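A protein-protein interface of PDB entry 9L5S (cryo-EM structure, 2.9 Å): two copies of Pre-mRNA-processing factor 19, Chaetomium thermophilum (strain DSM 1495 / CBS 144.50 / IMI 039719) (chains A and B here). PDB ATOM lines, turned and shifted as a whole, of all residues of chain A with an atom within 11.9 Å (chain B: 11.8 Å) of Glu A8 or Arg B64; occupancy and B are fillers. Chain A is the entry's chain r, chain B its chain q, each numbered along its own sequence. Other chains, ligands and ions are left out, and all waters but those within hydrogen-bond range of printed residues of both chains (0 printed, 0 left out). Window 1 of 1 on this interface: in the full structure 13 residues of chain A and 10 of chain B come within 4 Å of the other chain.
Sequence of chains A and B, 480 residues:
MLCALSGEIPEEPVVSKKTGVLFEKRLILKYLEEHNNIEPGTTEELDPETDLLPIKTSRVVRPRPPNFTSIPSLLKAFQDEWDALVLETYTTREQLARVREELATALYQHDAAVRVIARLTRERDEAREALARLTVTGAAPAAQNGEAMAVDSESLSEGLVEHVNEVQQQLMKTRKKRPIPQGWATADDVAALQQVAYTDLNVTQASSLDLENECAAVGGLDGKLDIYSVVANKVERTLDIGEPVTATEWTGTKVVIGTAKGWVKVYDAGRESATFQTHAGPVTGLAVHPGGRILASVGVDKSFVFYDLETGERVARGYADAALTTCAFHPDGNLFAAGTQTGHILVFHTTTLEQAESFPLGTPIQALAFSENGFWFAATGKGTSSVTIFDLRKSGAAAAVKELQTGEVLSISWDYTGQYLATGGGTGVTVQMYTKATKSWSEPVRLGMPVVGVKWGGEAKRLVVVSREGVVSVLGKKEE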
ATOM      1  N   MET A   1       5.315 -22.103 -15.337  1.00  0.00           N
ATOM      2  CA  MET A   1       6.474 -22.267 -16.205  1.00  0.00           C
ATOM      3  C   MET A   1       6.663 -21.049 -17.102  1.00  0.00           C
ATOM      4  O   MET A   1       5.713 -20.317 -17.381  1.00  0.00           O
ATOM      5  CB  MET A   1       6.332 -23.531 -17.057  1.00  0.00           C
ATOM      6  N   LEU A   2       7.898 -20.835 -17.550  1.00  0.00           N
ATOM      7  CA  LEU A   2       8.213 -19.709 -18.417  1.00  0.00           C
ATOM      8  C   LEU A   2       9.375 -20.088 -19.322  1.00  0.00           C
ATOM      9  O   LEU A   2      10.148 -21.004 -19.024  1.00  0.00           O
ATOM     10  CB  LEU A   2       8.550 -18.450 -17.608  1.00  0.00           C
ATOM     11  N   CYS A   3       9.484 -19.375 -20.440  1.00  0.00           N
ATOM     12  CA  CYS A   3      10.578 -19.602 -21.373  1.00  0.00           C
ATOM     13  C   CYS A   3      11.899 -19.138 -20.772  1.00  0.00           C
ATOM     14  O   CYS A   3      11.967 -18.105 -20.103  1.00  0.00           O
ATOM     15  CB  CYS A   3      10.314 -18.872 -22.689  1.00  0.00           C
ATOM     16  N   ALA A   4      12.955 -19.920 -21.008  1.00  0.00           N
ATOM     17  CA  ALA A   4      14.264 -19.569 -20.469  1.00  0.00           C
ATOM     18  C   ALA A   4      14.878 -18.379 -21.196  1.00  0.00           C
ATOM     19  O   ALA A   4      15.689 -17.651 -20.615  1.00  0.00           O
ATOM     20  CB  ALA A   4      15.202 -20.773 -20.540  1.00  0.00           C
ATOM     21  N   LEU A   5      14.508 -18.166 -22.461  1.00  0.00           N
ATOM     22  CA  LEU A   5      15.110 -17.095 -23.247  1.00  0.00           C
ATOM     23  C   LEU A   5      14.595 -15.719 -22.835  1.00  0.00           C
ATOM     24  O   LEU A   5      15.379 -14.769 -22.728  1.00  0.00           O
ATOM     25  CB  LEU A   5      14.855 -17.331 -24.736  1.00  0.00           C
ATOM     26  N   SER A   6      13.288 -15.590 -22.597  1.00  0.00           N
ATOM     27  CA  SER A   6      12.681 -14.290 -22.345  1.00  0.00           C
ATOM     28  C   SER A   6      12.068 -14.141 -20.961  1.00  0.00           C
ATOM     29  O   SER A   6      11.879 -13.007 -20.511  1.00  0.00           O
ATOM     30  CB  SER A   6      11.597 -13.998 -23.394  1.00  0.00           C
ATOM     31  N   GLY A   7      11.756 -15.240 -20.278  1.00  0.00           N
ATOM     32  CA  GLY A   7      11.104 -15.169 -18.988  1.00  0.00           C
ATOM     33  C   GLY A   7       9.596 -15.070 -19.033  1.00  0.00           C
ATOM     34  O   GLY A   7       8.972 -14.913 -17.976  1.00  0.00           O
ATOM     35  N   GLU A   8       8.990 -15.157 -20.213  1.00  0.00           N
ATOM     36  CA  GLU A   8       7.546 -15.100 -20.379  1.00  0.00           C
ATOM     37  C   GLU A   8       7.033 -16.441 -20.893  1.00  0.00           C
ATOM     38  O   GLU A   8       7.783 -17.411 -21.036  1.00  0.00           O
ATOM     39  CB  GLU A   8       7.160 -13.961 -21.327  1.00  0.00           C
ATOM     40  N   ILE A   9       5.734 -16.491 -21.172  1.00  0.00           N
ATOM     41  CA  ILE A   9       5.101 -17.703 -21.683  1.00  0.00           C
ATOM     42  C   ILE A   9       5.446 -17.852 -23.160  1.00  0.00           C
ATOM     43  O   ILE A   9       5.129 -16.962 -23.963  1.00  0.00           O
ATOM     44  CB  ILE A   9       3.580 -17.673 -21.469  1.00  0.00           C
ATOM     45  N   PRO A  10       6.086 -18.948 -23.563  1.00  0.00           N
ATOM     46  CA  PRO A  10       6.429 -19.120 -24.979  1.00  0.00           C
ATOM     47  C   PRO A  10       5.219 -19.527 -25.805  1.00  0.00           C
ATOM     48  O   PRO A  10       4.409 -20.360 -25.392  1.00  0.00           O
ATOM     49  CB  PRO A  10       7.485 -20.232 -24.954  1.00  0.00           C
ATOM     50  N   GLU A  11       5.099 -18.913 -26.986  1.00  0.00           N
ATOM     51  CA  GLU A  11       4.022 -19.272 -27.904  1.00  0.00           C
ATOM     52  C   GLU A  11       4.208 -20.681 -28.450  1.00  0.00           C
ATOM     53  O   GLU A  11       3.235 -21.429 -28.603  1.00  0.00           O
ATOM     54  CB  GLU A  11       3.947 -18.258 -29.045  1.00  0.00           C
ATOM     55  N   GLU A  12       5.450 -21.062 -28.747  1.00  0.00           N
ATOM     56  CA  GLU A  12       5.782 -22.399 -29.237  1.00  0.00           C
ATOM     57  C   GLU A  12       6.880 -22.956 -28.343  1.00  0.00           C
ATOM     58  O   GLU A  12       8.070 -22.886 -28.683  1.00  0.00           O
ATOM     59  CB  GLU A  12       6.215 -22.365 -30.701  1.00  0.00           C
ATOM     60  N   PRO A  13       6.520 -23.510 -27.187  1.00  0.00           N
ATOM     61  CA  PRO A  13       7.547 -23.991 -26.255  1.00  0.00           C
ATOM     62  C   PRO A  13       8.190 -25.282 -26.738  1.00  0.00           C
ATOM     63  O   PRO A  13       7.510 -26.263 -27.048  1.00  0.00           O
ATOM     64  CB  PRO A  13       6.768 -24.209 -24.952  1.00  0.00           C
ATOM     65  N   VAL A  14       9.519 -25.267 -26.800  1.00  0.00           N
ATOM     66  CA  VAL A  14      10.313 -26.425 -27.182  1.00  0.00           C
ATOM     67  C   VAL A  14      11.382 -26.637 -26.122  1.00  0.00           C
ATOM     68  O   VAL A  14      11.967 -25.681 -25.602  1.00  0.00           O
ATOM     69  CB  VAL A  14      10.952 -26.259 -28.578  1.00  0.00           C
ATOM     70  N   VAL A  21      15.555 -27.653 -21.118  1.00  0.00           N
ATOM     71  CA  VAL A  21      15.207 -26.251 -20.914  1.00  0.00           C
ATOM     72  C   VAL A  21      14.186 -25.839 -21.963  1.00  0.00           C
ATOM     73  O   VAL A  21      14.438 -25.948 -23.169  1.00  0.00           O
ATOM     74  CB  VAL A  21      16.458 -25.360 -20.981  1.00  0.00           C
ATOM     75  N   LEU A  22      13.030 -25.364 -21.506  1.00  0.00           N
ATOM     76  CA  LEU A  22      11.971 -24.940 -22.411  1.00  0.00           C
ATOM     77  C   LEU A  22      12.156 -23.481 -22.806  1.00  0.00           C
ATOM     78  O   LEU A  22      12.476 -22.630 -21.970  1.00  0.00           O
ATOM     79  CB  LEU A  22      10.601 -25.138 -21.760  1.00  0.00           C
ATOM     80  N   PHE A  23      11.946 -23.196 -24.088  1.00  0.00           N
ATOM     81  CA  PHE A  23      12.106 -21.846 -24.612  1.00  0.00           C
ATOM     82  C   PHE A  23      11.268 -21.707 -25.875  1.00  0.00           C
ATOM     83  O   PHE A  23      10.777 -22.692 -26.431  1.00  0.00           O
ATOM     84  CB  PHE A  23      13.577 -21.524 -24.891  1.00  0.00           C
ATOM     85  N   GLU A  24      11.102 -20.462 -26.315  1.00  0.00           N
ATOM     86  CA  GLU A  24      10.402 -20.193 -27.563  1.00  0.00           C
ATOM     87  C   GLU A  24      11.204 -20.722 -28.747  1.00  0.00           C
ATOM     88  O   GLU A  24      12.437 -20.698 -28.750  1.00  0.00           O
ATOM     89  CB  GLU A  24      10.153 -18.693 -27.725  1.00  0.00           C
ATOM     90  N   LYS A  25      10.482 -21.217 -29.758  1.00  0.00           N
ATOM     91  CA  LYS A  25      11.129 -21.849 -30.905  1.00  0.00           C
ATOM     92  C   LYS A  25      11.933 -20.846 -31.725  1.00  0.00           C
ATOM     93  O   LYS A  25      13.058 -21.142 -32.146  1.00  0.00           O
ATOM     94  CB  LYS A  25      10.083 -22.541 -31.781  1.00  0.00           C
ATOM     95  N   ARG A  26      11.372 -19.657 -31.962  1.00  0.00           N
ATOM     96  CA  ARG A  26      12.092 -18.632 -32.714  1.00  0.00           C
ATOM     97  C   ARG A  26      13.304 -18.125 -31.942  1.00  0.00           C
ATOM     98  O   ARG A  26      14.375 -17.917 -32.525  1.00  0.00           O
ATOM     99  CB  ARG A  26      11.151 -17.477 -33.058  1.00  0.00           C
ATOM    100  N   LEU A  27      13.153 -17.927 -30.629  1.00  0.00           N
ATOM    101  CA  LEU A  27      14.275 -17.485 -29.805  1.00  0.00           C
ATOM    102  C   LEU A  27      15.370 -18.543 -29.738  1.00  0.00           C
ATOM    103  O   LEU A  27      16.561 -18.213 -29.795  1.00  0.00           O
ATOM    104  CB  LEU A  27      13.785 -17.131 -28.401  1.00  0.00           C
ATOM    105  N   ILE A  28      14.987 -19.818 -29.631  1.00  0.00           N
ATOM    106  CA  ILE A  28      15.972 -20.895 -29.594  1.00  0.00           C
ATOM    107  C   ILE A  28      16.685 -21.018 -30.935  1.00  0.00           C
ATOM    108  O   ILE A  28      17.896 -21.263 -30.986  1.00  0.00           O
ATOM    109  CB  ILE A  28      15.309 -22.222 -29.185  1.00  0.00           C
ATOM    110  N   ILE A  55       6.442 -28.776 -27.382  1.00  0.00           N
ATOM    111  CA  ILE A  55       5.478 -29.111 -26.340  1.00  0.00           C
ATOM    112  C   ILE A  55       4.090 -28.754 -26.853  1.00  0.00           C
ATOM    113  O   ILE A  55       3.828 -27.593 -27.192  1.00  0.00           O
ATOM    114  CB  ILE A  55       5.780 -28.381 -25.022  1.00  0.00           C
ATOM    115  N   ARG A  59      -3.462 -23.436 -25.392  1.00  0.00           N
ATOM    116  CA  ARG A  59      -2.943 -22.084 -25.533  1.00  0.00           C
ATOM    117  C   ARG A  59      -3.190 -21.279 -24.263  1.00  0.00           C
ATOM    118  O   ARG A  59      -4.255 -21.369 -23.646  1.00  0.00           O
ATOM    119  CB  ARG A  59      -3.590 -21.388 -26.730  1.00  0.00           C
ATOM    120  N   VAL A  60      -2.195 -20.486 -23.876  1.00  0.00           N
ATOM    121  CA  VAL A  60      -2.300 -19.658 -22.680  1.00  0.00           C
ATOM    122  C   VAL A  60      -3.102 -18.407 -23.012  1.00  0.00           C
ATOM    123  O   VAL A  60      -2.787 -17.686 -23.966  1.00  0.00           O
ATOM    124  CB  VAL A  60      -0.905 -19.297 -22.144  1.00  0.00           C
ATOM    125  N   VAL A  61      -4.142 -18.149 -22.226  1.00  0.00           N
ATOM    126  CA  VAL A  61      -5.012 -16.998 -22.436  1.00  0.00           C
ATOM    127  C   VAL A  61      -4.476 -15.845 -21.596  1.00  0.00           C
ATOM    128  O   VAL A  61      -4.508 -15.892 -20.364  1.00  0.00           O
ATOM    129  CB  VAL A  61      -6.468 -17.319 -22.077  1.00  0.00           C
ATOM    130  N   ARG A  62      -3.980 -14.810 -22.264  1.00  0.00           N
ATOM    131  CA  ARG A  62      -3.456 -13.644 -21.563  1.00  0.00           C
ATOM    132  C   ARG A  62      -4.605 -12.808 -21.009  1.00  0.00           C
ATOM    133  O   ARG A  62      -5.643 -12.682 -21.667  1.00  0.00           O
ATOM    134  CB  ARG A  62      -2.596 -12.798 -22.497  1.00  0.00           C
ATOM    135  N   PRO A  63      -4.462 -12.229 -19.817  1.00  0.00           N
ATOM    136  CA  PRO A  63      -5.535 -11.382 -19.282  1.00  0.00           C
ATOM    137  C   PRO A  63      -5.548 -10.025 -19.970  1.00  0.00           C
ATOM    138  O   PRO A  63      -4.566  -9.281 -19.927  1.00  0.00           O
ATOM    139  CB  PRO A  63      -5.184 -11.259 -17.794  1.00  0.00           C
ATOM    140  N   GLU A  81       5.580  -0.085 -23.574  1.00  0.00           N
ATOM    141  CA  GLU A  81       6.302  -1.325 -23.301  1.00  0.00           C
ATOM    142  C   GLU A  81       7.658  -1.346 -23.996  1.00  0.00           C
ATOM    143  O   GLU A  81       8.646  -1.814 -23.420  1.00  0.00           O
ATOM    144  CB  GLU A  81       5.460  -2.526 -23.730  1.00  0.00           C
ATOM    145  N   ALA A  84       9.925   1.006 -22.057  1.00  0.00           N
ATOM    146  CA  ALA A  84      10.317   0.367 -20.806  1.00  0.00           C
ATOM    147  C   ALA A  84      11.349  -0.730 -21.040  1.00  0.00           C
ATOM    148  O   ALA A  84      12.284  -0.883 -20.247  1.00  0.00           O
ATOM    149  CB  ALA A  84       9.087  -0.196 -20.095  1.00  0.00           C
ATOM    150  N   LEU A  85      11.197  -1.498 -22.123  1.00  0.00           N
ATOM    151  CA  LEU A  85      12.174  -2.534 -22.451  1.00  0.00           C
ATOM    152  C   LEU A  85      13.529  -1.933 -22.803  1.00  0.00           C
ATOM    153  O   LEU A  85      14.572  -2.463 -22.399  1.00  0.00           O
ATOM    154  CB  LEU A  85      11.655  -3.397 -23.600  1.00  0.00           C
ATOM    155  N   GLU A  88      15.064  -0.714 -19.567  1.00  0.00           N
ATOM    156  CA  GLU A  88      15.522  -1.860 -18.787  1.00  0.00           C
ATOM    157  C   GLU A  88      16.806  -2.445 -19.360  1.00  0.00           C
ATOM    158  O   GLU A  88      17.697  -2.845 -18.603  1.00  0.00           O
ATOM    159  CB  GLU A  88      14.427  -2.923 -18.728  1.00  0.00           C
ATOM    160  N   MET B   1       0.006 -23.563 -20.364  1.00  0.00           N
ATOM    161  CA  MET B   1       0.743 -24.771 -20.015  1.00  0.00           C
ATOM    162  C   MET B   1       0.123 -25.458 -18.803  1.00  0.00           C
ATOM    163  O   MET B   1       0.037 -24.875 -17.724  1.00  0.00           O
ATOM    164  CB  MET B   1       2.213 -24.445 -19.742  1.00  0.00           C
ATOM    165  N   LYS B  56      12.989 -28.330 -16.828  1.00  0.00           N
ATOM    166  CA  LYS B  56      13.728 -27.473 -15.912  1.00  0.00           C
ATOM    167  C   LYS B  56      13.527 -26.017 -16.312  1.00  0.00           C
ATOM    168  O   LYS B  56      13.699 -25.661 -17.483  1.00  0.00           O
ATOM    169  CB  LYS B  56      15.217 -27.823 -15.914  1.00  0.00           C
ATOM    170  N   THR B  57      13.164 -25.184 -15.342  1.00  0.00           N
ATOM    171  CA  THR B  57      12.911 -23.768 -15.573  1.00  0.00           C
ATOM    172  C   THR B  57      14.086 -22.956 -15.043  1.00  0.00           C
ATOM    173  O   THR B  57      14.467 -23.097 -13.875  1.00  0.00           O
ATOM    174  CB  THR B  57      11.610 -23.327 -14.900  1.00  0.00           C
ATOM    175  N   SER B  58      14.654 -22.113 -15.899  1.00  0.00           N
ATOM    176  CA  SER B  58      15.777 -21.259 -15.537  1.00  0.00           C
ATOM    177  C   SER B  58      15.268 -19.863 -15.205  1.00  0.00           C
ATOM    178  O   SER B  58      14.466 -19.295 -15.954  1.00  0.00           O
ATOM    179  CB  SER B  58      16.802 -21.195 -16.671  1.00  0.00           C
ATOM    180  N   ARG B  59      15.736 -19.316 -14.085  1.00  0.00           N
ATOM    181  CA  ARG B  59      15.334 -17.988 -13.620  1.00  0.00           C
ATOM    182  C   ARG B  59      16.421 -16.949 -13.858  1.00  0.00           C
ATOM    183  O   ARG B  59      16.613 -16.042 -13.044  1.00  0.00           O
ATOM    184  CB  ARG B  59      14.954 -18.040 -12.144  1.00  0.00           C
ATOM    185  N   VAL B  60      17.158 -17.071 -14.964  1.00  0.00           N
ATOM    186  CA  VAL B  60      18.212 -16.109 -15.271  1.00  0.00           C
ATOM    187  C   VAL B  60      17.616 -14.762 -15.664  1.00  0.00           C
ATOM    188  O   VAL B  60      18.079 -13.707 -15.214  1.00  0.00           O
ATOM    189  CB  VAL B  60      19.137 -16.661 -16.370  1.00  0.00           C
ATOM    190  N   VAL B  61      16.586 -14.772 -16.505  1.00  0.00           N
ATOM    191  CA  VAL B  61      15.969 -13.544 -16.981  1.00  0.00           C
ATOM    192  C   VAL B  61      14.864 -13.126 -16.020  1.00  0.00           C
ATOM    193  O   VAL B  61      14.386 -13.911 -15.197  1.00  0.00           O
ATOM    194  CB  VAL B  61      15.425 -13.704 -18.415  1.00  0.00           C
ATOM    195  N   ARG B  62      14.461 -11.861 -16.120  1.00  0.00           N
ATOM    196  CA  ARG B  62      13.380 -11.353 -15.294  1.00  0.00           C
ATOM    197  C   ARG B  62      12.046 -11.956 -15.734  1.00  0.00           C
ATOM    198  O   ARG B  62      11.819 -12.184 -16.925  1.00  0.00           O
ATOM    199  CB  ARG B  62      13.312  -9.831 -15.376  1.00  0.00           C
ATOM    200  N   PRO B  63      11.145 -12.224 -14.787  1.00  0.00           N
ATOM    201  CA  PRO B  63       9.869 -12.861 -15.143  1.00  0.00           C
ATOM    202  C   PRO B  63       8.892 -11.850 -15.727  1.00  0.00           C
ATOM    203  O   PRO B  63       8.629 -10.803 -15.131  1.00  0.00           O
ATOM    204  CB  PRO B  63       9.364 -13.420 -13.808  1.00  0.00           C
ATOM    205  N   ARG B  64       8.354 -12.172 -16.902  1.00  0.00           N
ATOM    206  CA  ARG B  64       7.350 -11.346 -17.556  1.00  0.00           C
ATOM    207  C   ARG B  64       5.998 -12.034 -17.466  1.00  0.00           C
ATOM    208  O   ARG B  64       5.829 -13.122 -18.038  1.00  0.00           O
ATOM    209  CB  ARG B  64       7.724 -11.090 -19.015  1.00  0.00           C
ATOM    210  N   PRO B  65       5.024 -11.460 -16.755  1.00  0.00           N
ATOM    211  CA  PRO B  65       3.722 -12.115 -16.646  1.00  0.00           C
ATOM    212  C   PRO B  65       2.975 -12.061 -17.965  1.00  0.00           C
ATOM    213  O   PRO B  65       3.188 -11.146 -18.780  1.00  0.00           O
ATOM    214  CB  PRO B  65       3.004 -11.295 -15.559  1.00  0.00           C
ATOM    215  N   PRO B  66       2.085 -13.021 -18.223  1.00  0.00           N
ATOM    216  CA  PRO B  66       1.333 -13.039 -19.491  1.00  0.00           C
ATOM    217  C   PRO B  66       0.105 -12.132 -19.453  1.00  0.00           C
ATOM    218  O   PRO B  66      -1.042 -12.585 -19.496  1.00  0.00           O
ATOM    219  CB  PRO B  66       0.969 -14.523 -19.633  1.00  0.00           C
ATOM    220  N   ASN B  67       0.347 -10.830 -19.369  1.00  0.00           N
ATOM    221  CA  ASN B  67      -0.711  -9.833 -19.355  1.00  0.00           C
ATOM    222  C   ASN B  67      -0.859  -9.198 -20.735  1.00  0.00           C
ATOM    223  O   ASN B  67      -0.139  -9.522 -21.681  1.00  0.00           O
ATOM    224  CB  ASN B  67      -0.427  -8.760 -18.298  1.00  0.00           C
ATOM    225  N   PHE B  68      -1.818  -8.274 -20.838  1.00  0.00           N
ATOM    226  CA  PHE B  68      -2.049  -7.577 -22.097  1.00  0.00           C
ATOM    227  C   PHE B  68      -0.991  -6.517 -22.378  1.00  0.00           C
ATOM    228  O   PHE B  68      -0.873  -6.068 -23.524  1.00  0.00           O
ATOM    229  CB  PHE B  68      -3.438  -6.937 -22.097  1.00  0.00           C
ATOM    230  N   THR B  69      -0.224  -6.110 -21.368  1.00  0.00           N
ATOM    231  CA  THR B  69       0.798  -5.085 -21.537  1.00  0.00           C
ATOM    232  C   THR B  69       2.114  -5.636 -22.070  1.00  0.00           C
ATOM    233  O   THR B  69       3.038  -4.852 -22.315  1.00  0.00           O
ATOM    234  CB  THR B  69       1.047  -4.366 -20.208  1.00  0.00           C
ATOM    235  N   SER B  70       2.228  -6.950 -22.246  1.00  0.00           N
ATOM    236  CA  SER B  70       3.447  -7.538 -22.780  1.00  0.00           C
ATOM    237  C   SER B  70       3.614  -7.186 -24.255  1.00  0.00           C
ATOM    238  O   SER B  70       2.639  -7.045 -24.998  1.00  0.00           O
ATOM    239  CB  SER B  70       3.431  -9.056 -22.602  1.00  0.00           C
ATOM    240  N   ILE B  71       4.876  -7.024 -24.667  1.00  0.00           N
ATOM    241  CA  ILE B  71       5.167  -6.715 -26.068  1.00  0.00           C
ATOM    242  C   ILE B  71       4.767  -7.856 -26.995  1.00  0.00           C
ATOM    243  O   ILE B  71       4.143  -7.586 -28.035  1.00  0.00           O
ATOM    244  CB  ILE B  71       6.647  -6.322 -26.224  1.00  0.00           C
ATOM    245  N   PRO B  72       5.106  -9.119 -26.713  1.00  0.00           N
ATOM    246  CA  PRO B  72       4.611 -10.212 -27.569  1.00  0.00           C
ATOM    247  C   PRO B  72       3.099 -10.357 -27.549  1.00  0.00           C
ATOM    248  O   PRO B  72       2.498 -10.674 -28.583  1.00  0.00           O
ATOM    249  CB  PRO B  72       5.312 -11.449 -26.989  1.00  0.00           C
ATOM    250  N   SER B  73       2.465 -10.110 -26.399  1.00  0.00           N
ATOM    251  CA  SER B  73       1.007 -10.161 -26.327  1.00  0.00           C
ATOM    252  C   SER B  73       0.374  -9.038 -27.142  1.00  0.00           C
ATOM    253  O   SER B  73      -0.633  -9.253 -27.826  1.00  0.00           O
ATOM    254  CB  SER B  73       0.550 -10.092 -24.871  1.00  0.00           C
ATOM    255  N   LEU B  74       0.955  -7.836 -27.081  1.00  0.00           N
ATOM    256  CA  LEU B  74       0.462  -6.726 -27.892  1.00  0.00           C
ATOM    257  C   LEU B  74       0.658  -6.997 -29.378  1.00  0.00           C
ATOM    258  O   LEU B  74      -0.212  -6.666 -30.193  1.00  0.00           O
ATOM    259  CB  LEU B  74       1.159  -5.428 -27.487  1.00  0.00           C
ATOM    260  N   LYS B  76       0.742 -10.004 -30.783  1.00  0.00           N
ATOM    261  CA  LYS B  76      -0.234 -11.028 -31.145  1.00  0.00           C
ATOM    262  C   LYS B  76      -1.636 -10.442 -31.273  1.00  0.00           C
ATOM    263  O   LYS B  76      -2.389 -10.815 -32.181  1.00  0.00           O
ATOM    264  CB  LYS B  76      -0.216 -12.158 -30.116  1.00  0.00           C
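The backbone NH of Arg B64 is in hydrogen-bond range of the backbone carbonyl oxygen of Gly A7 (3.0 Å). The backbone NH of Phe B68 is in hydrogen-bond range of the backbone carbonyl oxygen of Pro A63, at 3.1 Å. The backbone nitrogen (N) of Pro A63 sits close to the backbone carbonyl oxygen (O) of Pro B66 (3.5 Å).
O of Glu A8 lies within hydrogen-bond range of N of Cys A3 (2.7 Å).
Among the printed residues, merely in contact across the chains: Arg A62 with Pro B66, Glu A8 with Arg B64, Gly A7 with Pro B63, Glu A81 with Thr B69, Ser A6 with Arg B62, Gly A7 with Arg B62, Val A21 with Lys B56 and Pro A63 with Asn B67.
Arg B64 touches just these residues of chain A: Gly A7 and Glu A8. No residue of chain B comes within 4 Å of Leu A2. No residue of chain B comes within 4 Å of Cys A3. No residue of chain B comes within 4 Å of Leu A5. Of chain B, only Arg B62 comes within 4 Å of Ser A6. Gly A7 touches just these residues of chain B: Arg B62 (3.7 Å), Pro B63 (3.6 Å) and Arg B64 (3.0 Å). No residue of chain B comes within 4 Å of Ile A9. No residue of chain B comes within 4 Å of Pro A10. Arg B62 touches two residues of chain A. No residue of chain A comes within 4 Å of Pro B65. Pro B66 touches just these residues of chain A: Arg A62 and Pro A63. Of the printed residues of chain B, Pro A63 touches Pro B66 (3.5 Å), Asn B67 (3.8 Å) and Phe B68 (3.1 Å). Printed residues of chain A within 4 Å of Lys B56: Val A21 (3.8 Å). Of the printed residues of chain B, Glu A81 touches Thr B69 (3.6 Å). Of the printed residues of chain A, Phe B68 touches Pro A63. The nearest residue of chain B that does not touch Glu A8 is Arg B62 (5.3 Å). The nearest residue of chain A that does not touch Arg B64 is Ile A9 (4.6 Å).
Among the printed residues, no Asp or Glu carboxylate lies within 4 Å of a Lys or Arg side-chain nitrogen of the other chain.
Positions printed for both chains: 1, 59, 60, 61, 62 and 63. Of the 11 pairs that touch across the chains among the printed residues, none has its exchanged pair printed and touching as well.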
